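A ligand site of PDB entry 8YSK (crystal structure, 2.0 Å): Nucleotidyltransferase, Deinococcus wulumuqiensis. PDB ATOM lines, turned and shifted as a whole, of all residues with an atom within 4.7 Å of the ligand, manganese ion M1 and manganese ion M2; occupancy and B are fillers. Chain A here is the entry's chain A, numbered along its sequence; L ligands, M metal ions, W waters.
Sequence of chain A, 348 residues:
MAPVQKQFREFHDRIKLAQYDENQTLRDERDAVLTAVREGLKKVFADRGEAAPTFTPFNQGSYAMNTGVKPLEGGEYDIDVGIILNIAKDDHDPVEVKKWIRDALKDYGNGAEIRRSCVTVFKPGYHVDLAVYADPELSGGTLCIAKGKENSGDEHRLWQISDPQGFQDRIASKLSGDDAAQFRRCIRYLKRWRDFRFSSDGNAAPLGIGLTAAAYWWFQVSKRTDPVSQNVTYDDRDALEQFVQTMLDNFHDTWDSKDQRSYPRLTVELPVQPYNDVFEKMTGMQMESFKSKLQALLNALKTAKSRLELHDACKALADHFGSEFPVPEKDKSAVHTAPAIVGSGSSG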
ATOM      1  N   GLN A  60     -18.104 -13.403  -0.870  1.00  0.00           N
ATOM      2  CA  GLN A  60     -16.765 -13.836  -1.310  1.00  0.00           C
ATOM      3  C   GLN A  60     -15.939 -14.233  -0.095  1.00  0.00           C
ATOM      4  O   GLN A  60     -16.362 -13.923   1.051  1.00  0.00           O
ATOM      5  CB  GLN A  60     -16.045 -12.735  -2.079  1.00  0.00           C
ATOM      6  CG  GLN A  60     -16.604 -12.490  -3.470  1.00  0.00           C
ATOM      7  CD  GLN A  60     -15.600 -11.675  -4.253  1.00  0.00           C
ATOM      8  OE1 GLN A  60     -14.666 -11.101  -3.712  1.00  0.00           O
ATOM      9  NE2 GLN A  60     -15.819 -11.549  -5.541  1.00  0.00           N
ATOM     10  N   GLY A  61     -14.819 -14.894  -0.371  1.00  0.00           N
ATOM     11  CA  GLY A  61     -13.752 -15.177   0.604  1.00  0.00           C
ATOM     12  C   GLY A  61     -14.157 -16.203   1.622  1.00  0.00           C
ATOM     13  O   GLY A  61     -15.100 -17.001   1.387  1.00  0.00           O
ATOM     14  N   SER A  62     -13.426 -16.225   2.729  1.00  0.00           N
ATOM     15  CA  SER A  62     -13.494 -17.325   3.705  1.00  0.00           C
ATOM     16  C   SER A  62     -14.909 -17.396   4.309  1.00  0.00           C
ATOM     17  O   SER A  62     -15.338 -18.517   4.636  1.00  0.00           O
ATOM     18  CB  SER A  62     -12.432 -17.164   4.762  1.00  0.00           C
ATOM     19  OG  SER A  62     -12.575 -15.929   5.453  1.00  0.00           O
ATOM     20  N   MET A  65     -17.021 -19.363   1.989  1.00  0.00           N
ATOM     21  CA  MET A  65     -16.527 -20.745   1.740  1.00  0.00           C
ATOM     22  C   MET A  65     -16.518 -21.557   3.051  1.00  0.00           C
ATOM     23  O   MET A  65     -16.170 -22.726   2.986  1.00  0.00           O
ATOM     24  CB  MET A  65     -15.108 -20.691   1.159  1.00  0.00           C
ATOM     25  CG  MET A  65     -15.112 -20.119  -0.235  1.00  0.00           C
ATOM     26  SD  MET A  65     -13.526 -20.166  -1.086  1.00  0.00           S
ATOM     27  CE  MET A  65     -12.828 -18.664  -0.410  1.00  0.00           C
ATOM     28  N   THR A  67     -14.453 -21.219   5.644  1.00  0.00           N
ATOM     29  CA  THR A  67     -13.042 -21.445   6.022  1.00  0.00           C
ATOM     30  C   THR A  67     -12.549 -20.303   6.907  1.00  0.00           C
ATOM     31  O   THR A  67     -11.329 -20.117   6.967  1.00  0.00           O
ATOM     32  CB  THR A  67     -12.180 -21.544   4.776  1.00  0.00           C
ATOM     33  OG1 THR A  67     -12.418 -20.373   3.975  1.00  0.00           O
ATOM     34  CG2 THR A  67     -12.486 -22.811   4.000  1.00  0.00           C
ATOM     35  N   ASP A  78     -12.295  -9.701   8.121  1.00  0.00           N
ATOM     36  CA  ASP A  78     -12.103  -9.409   6.688  1.00  0.00           C
ATOM     37  C   ASP A  78     -13.369  -9.857   5.967  1.00  0.00           C
ATOM     38  O   ASP A  78     -13.467 -11.044   5.682  1.00  0.00           O
ATOM     39  CB  ASP A  78     -10.882 -10.131   6.157  1.00  0.00           C
ATOM     40  CG  ASP A  78     -10.652  -9.935   4.671  1.00  0.00           C
ATOM     41  OD1 ASP A  78     -10.897  -8.812   4.172  1.00  0.00           O
ATOM     42  OD2 ASP A  78     -10.240 -10.887   4.040  1.00  0.00           O
ATOM     43  N   ASP A  80     -15.338 -10.115   2.814  1.00  0.00           N
ATOM     44  CA  ASP A  80     -15.097 -10.096   1.352  1.00  0.00           C
ATOM     45  C   ASP A  80     -16.470 -10.141   0.683  1.00  0.00           C
ATOM     46  O   ASP A  80     -17.295 -10.972   1.078  1.00  0.00           O
ATOM     47  CB  ASP A  80     -14.164 -11.217   0.929  1.00  0.00           C
ATOM     48  CG  ASP A  80     -12.800 -11.163   1.606  1.00  0.00           C
ATOM     49  OD1 ASP A  80     -12.402 -12.199   2.183  1.00  0.00           O
ATOM     50  OD2 ASP A  80     -12.172 -10.098   1.579  1.00  0.00           O
ATOM     51  N   SER A 117      -7.061  -4.646  -6.332  1.00  0.00           N
ATOM     52  CA  SER A 117      -8.086  -5.684  -6.631  1.00  0.00           C
ATOM     53  C   SER A 117      -9.451  -5.338  -6.034  1.00  0.00           C
ATOM     54  O   SER A 117     -10.445  -6.072  -6.312  1.00  0.00           O
ATOM     55  CB  SER A 117      -7.615  -7.020  -6.143  1.00  0.00           C
ATOM     56  OG  SER A 117      -6.529  -7.467  -6.948  1.00  0.00           O
ATOM     57  N   ASP A 129     -13.737  -5.632   1.961  1.00  0.00           N
ATOM     58  CA  ASP A 129     -13.083  -5.645   0.647  1.00  0.00           C
ATOM     59  C   ASP A 129     -14.195  -5.889  -0.394  1.00  0.00           C
ATOM     60  O   ASP A 129     -14.753  -7.015  -0.396  1.00  0.00           O
ATOM     61  CB  ASP A 129     -11.985  -6.719   0.627  1.00  0.00           C
ATOM     62  CG  ASP A 129     -10.845  -6.436   1.597  1.00  0.00           C
ATOM     63  OD1 ASP A 129     -10.617  -5.250   1.898  1.00  0.00           O
ATOM     64  OD2 ASP A 129     -10.164  -7.413   2.008  1.00  0.00           O
ATOM     65  N   ALA A 131     -14.790  -6.294  -4.118  1.00  0.00           N
ATOM     66  CA  ALA A 131     -14.324  -6.589  -5.481  1.00  0.00           C
ATOM     67  C   ALA A 131     -15.388  -6.044  -6.423  1.00  0.00           C
ATOM     68  O   ALA A 131     -16.581  -6.199  -6.149  1.00  0.00           O
ATOM     69  CB  ALA A 131     -14.075  -8.062  -5.640  1.00  0.00           C
ATOM     70  N   ILE A 145     -13.139  -8.245 -13.266  1.00  0.00           N
ATOM     71  CA  ILE A 145     -12.893  -7.438 -12.042  1.00  0.00           C
ATOM     72  C   ILE A 145     -12.096  -6.188 -12.441  1.00  0.00           C
ATOM     73  O   ILE A 145     -11.240  -6.291 -13.356  1.00  0.00           O
ATOM     74  CB  ILE A 145     -12.150  -8.254 -10.967  1.00  0.00           C
ATOM     75  CG1 ILE A 145     -12.150  -7.517  -9.627  1.00  0.00           C
ATOM     76  CG2 ILE A 145     -10.737  -8.605 -11.420  1.00  0.00           C
ATOM     77  CD1 ILE A 145     -11.776  -8.363  -8.428  1.00  0.00           C
ATOM     78  N   ASP A 163     -13.204 -15.350 -11.848  1.00  0.00           N
ATOM     79  CA  ASP A 163     -14.171 -16.454 -11.659  1.00  0.00           C
ATOM     80  C   ASP A 163     -14.291 -16.780 -10.179  1.00  0.00           C
ATOM     81  O   ASP A 163     -14.050 -17.910  -9.787  1.00  0.00           O
ATOM     82  CB  ASP A 163     -13.768 -17.679 -12.468  1.00  0.00           C
ATOM     83  CG  ASP A 163     -14.845 -18.732 -12.496  1.00  0.00           C
ATOM     84  OD1 ASP A 163     -16.004 -18.434 -12.070  1.00  0.00           O
ATOM     85  OD2 ASP A 163     -14.540 -19.835 -12.958  1.00  0.00           O
ATOM     86  N   PRO A 164     -14.715 -15.810  -9.342  1.00  0.00           N
ATOM     87  CA  PRO A 164     -14.794 -16.002  -7.898  1.00  0.00           C
ATOM     88  C   PRO A 164     -15.781 -17.092  -7.510  1.00  0.00           C
ATOM     89  O   PRO A 164     -15.502 -17.887  -6.612  1.00  0.00           O
ATOM     90  CB  PRO A 164     -15.219 -14.618  -7.342  1.00  0.00           C
ATOM     91  CG  PRO A 164     -15.825 -13.895  -8.530  1.00  0.00           C
ATOM     92  CD  PRO A 164     -15.118 -14.453  -9.754  1.00  0.00           C
ATOM     93  N   PHE A 167     -14.221 -20.452  -8.282  1.00  0.00           N
ATOM     94  CA  PHE A 167     -13.236 -20.785  -7.222  1.00  0.00           C
ATOM     95  C   PHE A 167     -13.990 -21.323  -6.008  1.00  0.00           C
ATOM     96  O   PHE A 167     -13.586 -22.347  -5.449  1.00  0.00           O
ATOM     97  CB  PHE A 167     -12.386 -19.574  -6.844  1.00  0.00           C
ATOM     98  CG  PHE A 167     -11.341 -19.907  -5.820  1.00  0.00           C
ATOM     99  CD1 PHE A 167     -10.341 -20.821  -6.112  1.00  0.00           C
ATOM    100  CD2 PHE A 167     -11.383 -19.341  -4.555  1.00  0.00           C
ATOM    101  CE1 PHE A 167      -9.393 -21.153  -5.154  1.00  0.00           C
ATOM    102  CE2 PHE A 167     -10.403 -19.651  -3.622  1.00  0.00           C
ATOM    103  CZ  PHE A 167      -9.441 -20.580  -3.904  1.00  0.00           C
ATOM    104  N   LYS A 191      -4.366 -21.132   8.721  1.00  0.00           N
ATOM    105  CA  LYS A 191      -4.612 -19.671   8.845  1.00  0.00           C
ATOM    106  C   LYS A 191      -4.281 -19.196  10.260  1.00  0.00           C
ATOM    107  O   LYS A 191      -3.739 -18.101  10.387  1.00  0.00           O
ATOM    108  CB  LYS A 191      -6.053 -19.325   8.492  1.00  0.00           C
ATOM    109  CG  LYS A 191      -6.389 -19.395   7.026  1.00  0.00           C
ATOM    110  CD  LYS A 191      -7.758 -18.822   6.763  1.00  0.00           C
ATOM    111  CE  LYS A 191      -8.260 -19.008   5.358  1.00  0.00           C
ATOM    112  NZ  LYS A 191      -9.705 -18.679   5.301  1.00  0.00           N
ATOM    113  N   ARG A 194      -0.541 -19.073  10.411  1.00  0.00           N
ATOM    114  CA  ARG A 194      -0.163 -17.858   9.664  1.00  0.00           C
ATOM    115  C   ARG A 194      -0.250 -16.652  10.603  1.00  0.00           C
ATOM    116  O   ARG A 194       0.725 -15.905  10.685  1.00  0.00           O
ATOM    117  CB  ARG A 194      -1.048 -17.647   8.432  1.00  0.00           C
ATOM    118  CG  ARG A 194      -0.887 -16.263   7.811  1.00  0.00           C
ATOM    119  CD  ARG A 194      -2.064 -15.886   6.963  1.00  0.00           C
ATOM    120  NE  ARG A 194      -3.321 -15.770   7.687  1.00  0.00           N
ATOM    121  CZ  ARG A 194      -4.514 -15.686   7.083  1.00  0.00           C
ATOM    122  NH1 ARG A 194      -4.605 -15.790   5.773  1.00  0.00           N
ATOM    123  NH2 ARG A 194      -5.621 -15.566   7.788  1.00  0.00           N
ATOM    124  N   LEU A 207      -1.107 -15.274   2.033  1.00  0.00           N
ATOM    125  CA  LEU A 207      -2.536 -14.904   1.843  1.00  0.00           C
ATOM    126  C   LEU A 207      -3.428 -16.124   2.112  1.00  0.00           C
ATOM    127  O   LEU A 207      -3.077 -17.219   1.655  1.00  0.00           O
ATOM    128  CB  LEU A 207      -2.732 -14.422   0.395  1.00  0.00           C
ATOM    129  CG  LEU A 207      -2.169 -13.033   0.071  1.00  0.00           C
ATOM    130  CD1 LEU A 207      -2.494 -12.677  -1.366  1.00  0.00           C
ATOM    131  CD2 LEU A 207      -2.709 -11.962   1.021  1.00  0.00           C
ATOM    132  N   GLY A 208      -4.567 -15.921   2.790  1.00  0.00           N
ATOM    133  CA  GLY A 208      -5.620 -16.919   2.982  1.00  0.00           C
ATOM    134  C   GLY A 208      -5.910 -17.661   1.685  1.00  0.00           C
ATOM    135  O   GLY A 208      -5.954 -18.895   1.702  1.00  0.00           O
ATOM    136  N   ILE A 209      -6.089 -16.925   0.591  1.00  0.00           N
ATOM    137  CA  ILE A 209      -6.522 -17.541  -0.707  1.00  0.00           C
ATOM    138  C   ILE A 209      -5.419 -18.469  -1.211  1.00  0.00           C
ATOM    139  O   ILE A 209      -5.754 -19.481  -1.857  1.00  0.00           O
ATOM    140  CB  ILE A 209      -6.905 -16.472  -1.746  1.00  0.00           C
ATOM    141  CG1 ILE A 209      -7.500 -17.138  -2.994  1.00  0.00           C
ATOM    142  CG2 ILE A 209      -5.711 -15.587  -2.063  1.00  0.00           C
ATOM    143  CD1 ILE A 209      -8.168 -16.168  -3.955  1.00  0.00           C
ATOM    144  N   THR A 212      -5.632 -21.670   0.731  1.00  0.00           N
ATOM    145  CA  THR A 212      -6.893 -22.322   0.340  1.00  0.00           C
ATOM    146  C   THR A 212      -6.683 -22.988  -1.021  1.00  0.00           C
ATOM    147  O   THR A 212      -7.007 -24.148  -1.151  1.00  0.00           O
ATOM    148  CB  THR A 212      -8.054 -21.317   0.347  1.00  0.00           C
ATOM    149  OG1 THR A 212      -8.044 -20.718   1.647  1.00  0.00           O
ATOM    150  CG2 THR A 212      -9.390 -21.940   0.034  1.00  0.00           C
ATOM    151  N   LEU A 270      -4.155 -20.147  -9.164  1.00  0.00           N
ATOM    152  CA  LEU A 270      -5.620 -20.255  -9.012  1.00  0.00           C
ATOM    153  C   LEU A 270      -6.106 -21.355  -9.955  1.00  0.00           C
ATOM    154  O   LEU A 270      -5.635 -21.451 -11.086  1.00  0.00           O
ATOM    155  CB  LEU A 270      -6.240 -18.892  -9.324  1.00  0.00           C
ATOM    156  CG  LEU A 270      -7.512 -18.586  -8.566  1.00  0.00           C
ATOM    157  CD1 LEU A 270      -7.255 -18.545  -7.056  1.00  0.00           C
ATOM    158  CD2 LEU A 270      -8.124 -17.274  -9.056  1.00  0.00           C
ATOM    159  N   VAL A 272      -8.934 -21.482 -11.356  1.00  0.00           N
ATOM    160  CA  VAL A 272      -9.902 -20.843 -12.275  1.00  0.00           C
ATOM    161  C   VAL A 272      -9.239 -19.579 -12.829  1.00  0.00           C
ATOM    162  O   VAL A 272      -8.135 -19.222 -12.367  1.00  0.00           O
ATOM    163  CB  VAL A 272     -11.240 -20.523 -11.563  1.00  0.00           C
ATOM    164  CG1 VAL A 272     -11.933 -21.790 -11.038  1.00  0.00           C
ATOM    165  CG2 VAL A 272     -11.084 -19.510 -10.438  1.00  0.00           C
ATOM    166  N   GLN A 273      -9.861 -18.925 -13.805  1.00  0.00           N
ATOM    167  CA  GLN A 273      -9.396 -17.644 -14.376  1.00  0.00           C
ATOM    168  C   GLN A 273      -9.174 -16.669 -13.231  1.00  0.00           C
ATOM    169  O   GLN A 273     -10.003 -16.567 -12.337  1.00  0.00           O
ATOM    170  CB  GLN A 273     -10.432 -17.079 -15.357  1.00  0.00           C
ATOM    171  CG  GLN A 273     -10.551 -17.892 -16.637  1.00  0.00           C
ATOM    172  CD  GLN A 273      -9.481 -17.528 -17.632  1.00  0.00           C
ATOM    173  OE1 GLN A 273      -8.550 -16.796 -17.333  1.00  0.00           O
ATOM    174  NE2 GLN A 273      -9.587 -18.073 -18.838  1.00  0.00           N
HETATM  175  P1  LIG L   1      -8.487 -13.508   1.014  1.00  0.00           P
HETATM  176  O1  LIG L   1      -7.000 -13.590   1.134  1.00  0.00           O
HETATM  177  O2  LIG L   1      -9.344 -12.613   1.849  1.00  0.00           O
HETATM  178  O3  LIG L   1      -9.010 -15.003   1.111  1.00  0.00           O
HETATM  179  O4  LIG L   1      -8.869 -13.297  -0.491  1.00  0.00           O
HETATM  180  P2  LIG L   1      -9.956 -15.715   2.130  1.00  0.00           P
HETATM  181  O5  LIG L   1     -10.227 -17.093   1.611  1.00  0.00           O
HETATM  182  O6  LIG L   1     -11.078 -14.824   2.489  1.00  0.00           O
HETATM  183  O7  LIG L   1      -8.976 -15.877   3.377  1.00  0.00           O
HETATM  184  P3  LIG L   1      -8.826 -15.171   4.820  1.00  0.00           P
HETATM  185  O8  LIG L   1      -9.349 -13.787   4.578  1.00  0.00           O
HETATM  186  O9  LIG L   1      -7.367 -15.250   5.180  1.00  0.00           O
HETATM  187  O10 LIG L   1      -9.673 -15.980   5.729  1.00  0.00           O
HETATM  188  C1  LIG L   1     -10.224 -13.025  -0.830  1.00  0.00           C
HETATM  189  C2  LIG L   1     -10.144 -12.262  -2.110  1.00  0.00           C
HETATM  190  O11 LIG L   1      -9.704 -13.151  -3.144  1.00  0.00           O
HETATM  191  C3  LIG L   1      -9.979 -12.547  -4.373  1.00  0.00           C
HETATM  192  C4  LIG L   1     -11.167 -11.573  -4.165  1.00  0.00           C
HETATM  193  O12 LIG L   1     -10.826 -10.269  -4.617  1.00  0.00           O
HETATM  194  C5  LIG L   1     -11.432 -11.651  -2.645  1.00  0.00           C
HETATM  195  O13 LIG L   1     -11.596 -10.406  -1.988  1.00  0.00           O
HETATM  196  N1  LIG L   1     -10.271 -13.614  -5.329  1.00  0.00           N
HETATM  197  C6  LIG L   1      -9.531 -13.735  -6.486  1.00  0.00           C
HETATM  198  C7  LIG L   1     -11.317 -14.475  -5.041  1.00  0.00           C
HETATM  199  O14 LIG L   1     -11.990 -14.400  -4.017  1.00  0.00           O
HETATM  200  N2  LIG L   1     -11.562 -15.427  -6.009  1.00  0.00           N
HETATM  201  C8  LIG L   1     -10.887 -15.587  -7.198  1.00  0.00           C
HETATM  202  O15 LIG L   1     -11.232 -16.480  -7.969  1.00  0.00           O
HETATM  203  C9  LIG L   1      -9.811 -14.667  -7.412  1.00  0.00           C
HETATM  204 MN    MN M   1     -10.268  -9.448   2.171  1.00  0.00          MN
HETATM  205 MN    MN M   2     -10.830 -12.927   3.382  1.00  0.00          MN
HETATM  206  O   HOH W   1     -12.474 -13.282   4.738  1.00  0.00           O
HETATM  207  O   HOH W   2     -10.883 -15.344 -10.382  1.00  0.00           O
HETATM  208  O   HOH W   3      -5.521 -13.330   3.987  1.00  0.00           O
HETATM  209  O   HOH W   4     -10.277 -19.523   2.553  1.00  0.00           O
HETATM  210  O   HOH W   5      -8.126  -9.438   2.549  1.00  0.00           O
HETATM  211  O   HOH W   6     -13.887  -9.120  -1.866  1.00  0.00           O
HETATM  212  O   HOH W   7     -14.656 -15.621  -3.520  1.00  0.00           O
HETATM  213  O   HOH W   8     -12.130 -11.985  -7.564  1.00  0.00           O
HETATM  214  O   HOH W   9      -9.713  -9.828   0.252  1.00  0.00           O
HETATM  215  O   HOH W  10     -10.790 -15.864   8.215  1.00  0.00           O
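The side-chain amino group (NZ) of Lys 191 lies within salt-bridge range of an oxygen (O10) of the ligand (2.7 Å). The backbone NH of Ser 62 is in hydrogen-bond range of an oxygen (O5) of the ligand, at 3.5 Å. O10 of the ligand is in hydrogen-bond range of OG of Ser 62 (2.9 Å). NH1 of Arg 194 is in salt-bridge range of O9 of the ligand (2.9 Å). The backbone NH of Ile 209 sits at hydrogen-bond distance from an oxygen (O1) of the ligand.
The backbone carbonyl oxygen (O) of Asp 80 sits at hydrogen-bond distance from the backbone NH (N) of Gln 60 (3.2 Å). NZ of Lys 191 lies within hydrogen-bond range of O of Thr 67 (2.7 Å). O of Ser 62 is in hydrogen-bond range of N of Thr 67 (3.0 Å). The backbone carbonyl oxygen (O) of Gly 208 is in hydrogen-bond range of the side-chain hydroxyl (OG1) of Thr 212 (2.8 Å). N of Asp 163 lies within hydrogen-bond range of O of Gln 273, 3.5 Å away.
Residues that only touch the ligand: Gly 208, Gly 61, Leu 270, Gln 60, Phe 167, Pro 164, Asp 163, Met 65 and Val 272. Within 4 Å of the ligand: Gln 60, Gly 61, Ser 62, Met 65, Asp 78, Asp 80, Asp 163, Pro 164, Phe 167, Lys 191, Arg 194, Gly 208, Ile 209, Leu 270 and Val 272. The nearest printed residue that does not touch the ligand is Ala 131 (4.1 Å).
Three residues have an atom within 4 Å of manganese ion M1: Asp 78, Asp 80 and Asp 129. The nearest printed residue that does not touch manganese ion M1 is Gly 61 (6.9 Å).
The nearest printed residue that does not touch manganese ion M2 is Ser 62 (4.04 Å).
Manganese ion M1 is bound by water W9 (2.0 Å), OD2 of Asp 129 (2.0 Å), OD2 of Asp 80 (2.1 Å), water W5 (2.2 Å), OD1 of Asp 78 (2.2 Å) and OD2 of Asp 78 (2.4 Å).
An oxygen (O8) of the ligand binds manganese ion M2 (2.1 Å). OD1 of Asp 80 binds manganese ion M2 (2.1 Å). O6 of the ligand binds manganese ion M2 (2.1 Å). O2 of the ligand binds manganese ion M2 (2.2 Å). Water W1 binds manganese ion M2 (2.2 Å). The side-chain carboxylate (OD2) of Asp 78 is bound to manganese ion M2 (2.2 Å).
Water W1 lies within hydrogen-bond range of the backbone carbonyl oxygen (O) of Asp 78 (2.6 Å) and the side-chain hydroxyl (OG) of Ser 62 (2.7 Å). Water W4 lies within hydrogen-bond range of an oxygen (O5) of the ligand, the side-chain hydroxyl of Thr 212, the side-chain hydroxyl of Thr 67 and the side-chain amino group of Lys 191. Water W6 lies within hydrogen-bond range of an oxygen (O13) of the ligand (2.6 Å), the backbone carbonyl oxygen (O) of Asp 129 (2.7 Å) and the side-chain amide oxygen (OE1) of Gln 60 (2.8 Å). Water W10 lies within hydrogen-bond range of O10 of the ligand and OG of Ser 62. Water W3 lies within hydrogen-bond range of an oxygen (O9) of the ligand (2.9 Å), the backbone NH of Gly 208 (3.0 Å) and the guanidinium group of Arg 194 (3.2 Å). Water W7 lies within hydrogen-bond range of an oxygen (O14) of the ligand (3.0 Å) and the backbone NH of Gly 61 (3.2 Å).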
